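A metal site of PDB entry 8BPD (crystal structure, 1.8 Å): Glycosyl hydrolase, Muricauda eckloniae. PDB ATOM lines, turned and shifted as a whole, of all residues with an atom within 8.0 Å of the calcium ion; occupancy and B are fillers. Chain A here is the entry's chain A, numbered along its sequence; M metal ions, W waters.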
ATOM      1  N   VAL A 239      11.918   0.157   1.026  1.00  0.00           N
ATOM      2  CA  VAL A 239      12.998   0.377   0.081  1.00  0.00           C
ATOM      3  C   VAL A 239      12.899  -0.686  -1.006  1.00  0.00           C
ATOM      4  O   VAL A 239      12.696  -1.878  -0.710  1.00  0.00           O
ATOM      5  CB  VAL A 239      14.359   0.330   0.791  1.00  0.00           C
ATOM      6  CG1 VAL A 239      15.489   0.311  -0.224  1.00  0.00           C
ATOM      7  CG2 VAL A 239      14.482   1.528   1.738  1.00  0.00           C
ATOM      8  N   ASP A 240      12.996  -0.248  -2.251  1.00  0.00           N
ATOM      9  CA  ASP A 240      13.012  -1.125  -3.398  1.00  0.00           C
ATOM     10  C   ASP A 240      14.442  -1.469  -3.774  1.00  0.00           C
ATOM     11  O   ASP A 240      14.829  -2.642  -3.796  1.00  0.00           O
ATOM     12  CB  ASP A 240      12.282  -0.447  -4.560  1.00  0.00           C
ATOM     13  CG  ASP A 240      12.230  -1.292  -5.801  1.00  0.00           C
ATOM     14  OD1 ASP A 240      12.382  -2.528  -5.705  1.00  0.00           O
ATOM     15  OD2 ASP A 240      12.053  -0.713  -6.895  1.00  0.00           O
ATOM     16  N   SER A 241      15.256  -0.440  -3.977  1.00  0.00           N
ATOM     17  CA  SER A 241      16.631  -0.588  -4.414  1.00  0.00           C
ATOM     18  C   SER A 241      17.524   0.270  -3.547  1.00  0.00           C
ATOM     19  O   SER A 241      17.154   1.382  -3.167  1.00  0.00           O
ATOM     20  CB  SER A 241      16.840  -0.153  -5.859  1.00  0.00           C
ATOM     21  OG  SER A 241      18.239  -0.114  -6.143  1.00  0.00           O
ATOM     22  N   ASP A 242      18.701  -0.255  -3.247  1.00  0.00           N
ATOM     23  CA  ASP A 242      19.721   0.513  -2.563  1.00  0.00           C
ATOM     24  C   ASP A 242      20.656   1.228  -3.520  1.00  0.00           C
ATOM     25  O   ASP A 242      21.551   1.949  -3.071  1.00  0.00           O
ATOM     26  CB  ASP A 242      20.507  -0.402  -1.624  1.00  0.00           C
ATOM     27  CG  ASP A 242      19.659  -0.888  -0.498  1.00  0.00           C
ATOM     28  OD1 ASP A 242      19.326  -0.080   0.408  1.00  0.00           O
ATOM     29  OD2 ASP A 242      19.234  -2.072  -0.553  1.00  0.00           O
ATOM     30  N   GLY A 243      20.445   1.095  -4.813  1.00  0.00           N
ATOM     31  CA  GLY A 243      21.289   1.721  -5.810  1.00  0.00           C
ATOM     32  C   GLY A 243      21.437   0.820  -7.026  1.00  0.00           C
ATOM     33  O   GLY A 243      21.113  -0.365  -7.010  1.00  0.00           O
ATOM     34  N   ASN A 245      23.608  -0.837  -8.439  1.00  0.00           N
ATOM     35  CA  ASN A 245      24.255  -2.144  -8.295  1.00  0.00           C
ATOM     36  C   ASN A 245      23.931  -2.799  -6.946  1.00  0.00           C
ATOM     37  O   ASN A 245      24.766  -3.512  -6.379  1.00  0.00           O
ATOM     38  CB  ASN A 245      25.761  -2.002  -8.481  1.00  0.00           C
ATOM     39  CG  ASN A 245      26.123  -1.781  -9.941  1.00  0.00           C
ATOM     40  OD1 ASN A 245      26.224  -2.731 -10.719  1.00  0.00           O
ATOM     41  ND2 ASN A 245      26.318  -0.526 -10.313  1.00  0.00           N
ATOM     42  N   ASP A 246      22.736  -2.574  -6.449  1.00  0.00           N
ATOM     43  CA  ASP A 246      22.205  -3.260  -5.281  1.00  0.00           C
ATOM     44  C   ASP A 246      22.427  -4.769  -5.422  1.00  0.00           C
ATOM     45  O   ASP A 246      21.971  -5.365  -6.400  1.00  0.00           O
ATOM     46  CB  ASP A 246      20.712  -2.938  -5.166  1.00  0.00           C
ATOM     47  CG  ASP A 246      20.099  -3.367  -3.856  1.00  0.00           C
ATOM     48  OD1 ASP A 246      18.923  -3.016  -3.621  1.00  0.00           O
ATOM     49  OD2 ASP A 246      20.788  -4.053  -3.051  1.00  0.00           O
ATOM     50  N   PRO A 247      23.119  -5.416  -4.475  1.00  0.00           N
ATOM     51  CA  PRO A 247      23.393  -6.852  -4.610  1.00  0.00           C
ATOM     52  C   PRO A 247      22.268  -7.764  -4.151  1.00  0.00           C
ATOM     53  O   PRO A 247      22.327  -8.967  -4.413  1.00  0.00           O
ATOM     54  CB  PRO A 247      24.626  -7.040  -3.715  1.00  0.00           C
ATOM     55  CG  PRO A 247      24.444  -5.988  -2.655  1.00  0.00           C
ATOM     56  CD  PRO A 247      23.870  -4.806  -3.362  1.00  0.00           C
ATOM     57  N   ASP A 248      21.269  -7.216  -3.480  1.00  0.00           N
ATOM     58  CA  ASP A 248      20.191  -7.964  -2.853  1.00  0.00           C
ATOM     59  C   ASP A 248      18.908  -7.234  -3.222  1.00  0.00           C
ATOM     60  O   ASP A 248      18.711  -6.090  -2.815  1.00  0.00           O
ATOM     61  CB  ASP A 248      20.377  -7.988  -1.336  1.00  0.00           C
ATOM     62  CG  ASP A 248      19.415  -8.892  -0.621  1.00  0.00           C
ATOM     63  OD1 ASP A 248      18.369  -9.256  -1.184  1.00  0.00           O
ATOM     64  OD2 ASP A 248      19.711  -9.234   0.552  1.00  0.00           O
ATOM     65  N   GLY A 249      18.052  -7.864  -4.019  1.00  0.00           N
ATOM     66  CA  GLY A 249      16.859  -7.187  -4.486  1.00  0.00           C
ATOM     67  C   GLY A 249      15.713  -7.171  -3.519  1.00  0.00           C
ATOM     68  O   GLY A 249      14.634  -6.679  -3.846  1.00  0.00           O
ATOM     69  N   ARG A 250      15.891  -7.706  -2.319  1.00  0.00           N
ATOM     70  CA  ARG A 250      14.789  -7.811  -1.380  1.00  0.00           C
ATOM     71  C   ARG A 250      14.397  -6.416  -0.907  1.00  0.00           C
ATOM     72  O   ARG A 250      15.258  -5.591  -0.595  1.00  0.00           O
ATOM     73  CB  ARG A 250      15.186  -8.682  -0.210  1.00  0.00           C
ATOM     74  CG  ARG A 250      15.168 -10.191  -0.553  1.00  0.00           C
ATOM     75  CD  ARG A 250      15.503 -11.009   0.655  1.00  0.00           C
ATOM     76  NE  ARG A 250      16.880 -10.790   1.069  1.00  0.00           N
ATOM     77  CZ  ARG A 250      17.370 -11.121   2.260  1.00  0.00           C
ATOM     78  NH1 ARG A 250      16.601 -11.685   3.183  1.00  0.00           N
ATOM     79  NH2 ARG A 250      18.645 -10.868   2.530  1.00  0.00           N
ATOM     80  N   LYS A 251      13.093  -6.150  -0.887  1.00  0.00           N
ATOM     81  CA  LYS A 251      12.589  -4.906  -0.339  1.00  0.00           C
ATOM     82  C   LYS A 251      12.502  -5.020   1.171  1.00  0.00           C
ATOM     83  O   LYS A 251      12.358  -6.120   1.708  1.00  0.00           O
ATOM     84  CB  LYS A 251      11.209  -4.568  -0.901  1.00  0.00           C
ATOM     85  CG  LYS A 251      10.178  -5.607  -0.565  1.00  0.00           C
ATOM     86  CD  LYS A 251       8.782  -5.145  -0.930  1.00  0.00           C
ATOM     87  CE  LYS A 251       8.571  -5.138  -2.419  1.00  0.00           C
ATOM     88  NZ  LYS A 251       8.392  -6.502  -2.951  1.00  0.00           N
ATOM     89  N   TYR A 252      12.552  -3.881   1.845  1.00  0.00           N
ATOM     90  CA  TYR A 252      12.526  -3.897   3.294  1.00  0.00           C
ATOM     91  C   TYR A 252      11.915  -2.608   3.848  1.00  0.00           C
ATOM     92  O   TYR A 252      12.018  -1.542   3.235  1.00  0.00           O
ATOM     93  CB  TYR A 252      13.944  -4.130   3.830  1.00  0.00           C
ATOM     94  CG  TYR A 252      14.978  -3.104   3.424  1.00  0.00           C
ATOM     95  CD1 TYR A 252      15.774  -3.288   2.298  1.00  0.00           C
ATOM     96  CD2 TYR A 252      15.189  -1.971   4.195  1.00  0.00           C
ATOM     97  CE1 TYR A 252      16.746  -2.347   1.941  1.00  0.00           C
ATOM     98  CE2 TYR A 252      16.142  -1.031   3.849  1.00  0.00           C
ATOM     99  CZ  TYR A 252      16.914  -1.218   2.725  1.00  0.00           C
ATOM    100  OH  TYR A 252      17.871  -0.256   2.408  1.00  0.00           O
ATOM    101  N   TRP A 276      16.794  -9.566   6.746  1.00  0.00           N
ATOM    102  CA  TRP A 276      15.726  -9.228   5.815  1.00  0.00           C
ATOM    103  C   TRP A 276      16.248  -8.570   4.564  1.00  0.00           C
ATOM    104  O   TRP A 276      15.461  -8.312   3.653  1.00  0.00           O
ATOM    105  CB  TRP A 276      14.702  -8.286   6.435  1.00  0.00           C
ATOM    106  CG  TRP A 276      14.030  -8.757   7.657  1.00  0.00           C
ATOM    107  CD1 TRP A 276      14.202  -9.940   8.287  1.00  0.00           C
ATOM    108  CD2 TRP A 276      13.049  -8.029   8.427  1.00  0.00           C
ATOM    109  NE1 TRP A 276      13.409 -10.005   9.406  1.00  0.00           N
ATOM    110  CE2 TRP A 276      12.682  -8.845   9.514  1.00  0.00           C
ATOM    111  CE3 TRP A 276      12.452  -6.776   8.286  1.00  0.00           C
ATOM    112  CZ2 TRP A 276      11.750  -8.448  10.473  1.00  0.00           C
ATOM    113  CZ3 TRP A 276      11.523  -6.366   9.241  1.00  0.00           C
ATOM    114  CH2 TRP A 276      11.172  -7.205  10.311  1.00  0.00           C
ATOM    115  N   GLY A 277      17.544  -8.285   4.505  1.00  0.00           N
ATOM    116  CA  GLY A 277      18.128  -7.608   3.367  1.00  0.00           C
ATOM    117  C   GLY A 277      18.344  -6.121   3.558  1.00  0.00           C
ATOM    118  O   GLY A 277      18.762  -5.457   2.606  1.00  0.00           O
ATOM    119  N   ALA A 278      18.096  -5.580   4.749  1.00  0.00           N
ATOM    120  CA  ALA A 278      18.319  -4.171   5.041  1.00  0.00           C
ATOM    121  C   ALA A 278      19.790  -3.914   5.386  1.00  0.00           C
ATOM    122  O   ALA A 278      20.242  -4.307   6.459  1.00  0.00           O
ATOM    123  CB  ALA A 278      17.437  -3.741   6.209  1.00  0.00           C
ATOM    124  N   PRO A 279      20.561  -3.243   4.527  1.00  0.00           N
ATOM    125  CA  PRO A 279      21.959  -3.013   4.859  1.00  0.00           C
ATOM    126  C   PRO A 279      22.068  -2.021   5.998  1.00  0.00           C
ATOM    127  O   PRO A 279      21.225  -1.111   6.142  1.00  0.00           O
ATOM    128  CB  PRO A 279      22.536  -2.443   3.546  1.00  0.00           C
ATOM    129  CG  PRO A 279      21.400  -1.864   2.844  1.00  0.00           C
ATOM    130  CD  PRO A 279      20.202  -2.688   3.214  1.00  0.00           C
ATOM    131  N   TRP A 283      20.557   3.940   2.866  1.00  0.00           N
ATOM    132  CA  TRP A 283      20.262   5.339   2.604  1.00  0.00           C
ATOM    133  C   TRP A 283      19.000   5.763   3.313  1.00  0.00           C
ATOM    134  O   TRP A 283      18.852   6.936   3.699  1.00  0.00           O
ATOM    135  CB  TRP A 283      20.125   5.582   1.105  1.00  0.00           C
ATOM    136  CG  TRP A 283      18.987   4.853   0.422  1.00  0.00           C
ATOM    137  CD1 TRP A 283      19.046   3.631  -0.207  1.00  0.00           C
ATOM    138  CD2 TRP A 283      17.625   5.318   0.256  1.00  0.00           C
ATOM    139  NE1 TRP A 283      17.816   3.309  -0.721  1.00  0.00           N
ATOM    140  CE2 TRP A 283      16.932   4.331  -0.469  1.00  0.00           C
ATOM    141  CE3 TRP A 283      16.941   6.474   0.653  1.00  0.00           C
ATOM    142  CZ2 TRP A 283      15.586   4.447  -0.782  1.00  0.00           C
ATOM    143  CZ3 TRP A 283      15.609   6.589   0.320  1.00  0.00           C
ATOM    144  CH2 TRP A 283      14.938   5.576  -0.378  1.00  0.00           C
HETATM  145 CA    CA M   1      18.938  -4.182  -1.545  1.00  0.00          CA
HETATM  146  O   HOH W   1      17.735  -5.519   0.055  1.00  0.00           O
HETATM  147  O   HOH W   2      16.578  -3.795  -1.908  1.00  0.00           O
HETATM  148  O   HOH W   3      20.862  -4.642  -0.352  1.00  0.00           O
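The side-chain carboxylate of Asp 242 is in hydrogen-bond range of the side-chain hydroxyl of Tyr 252 (2.5 Å).
The guanidinium group (NH2) of Arg 250 is in salt-bridge range of the side-chain carboxylate (OD2) of Asp 248 (2.8 Å).
Water W2 bridges O of Arg 250 and O of Asp 240.
Water W1 bridges O of Arg 250 (2.6 Å) and O of Gly 277 (2.8 Å).
The calcium ion is bound by O of Asp 248 (2.3 Å), water W3 (2.3 Å), OD2 of Asp 242 (2.4 Å), OD1 of Asp 246 (2.4 Å), OD2 of Asp 246 (2.4 Å), water W1 (2.4 Å) and water W2 (2.4 Å).
The calcium ion has seven donor atoms within binding distance.
Three residues have an atom within 4 Å of the calcium ion: Asp 242, Asp 246 and Asp 248.
The nearest printed residue that does not touch the calcium ion is Arg 250 (4.1 Å).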
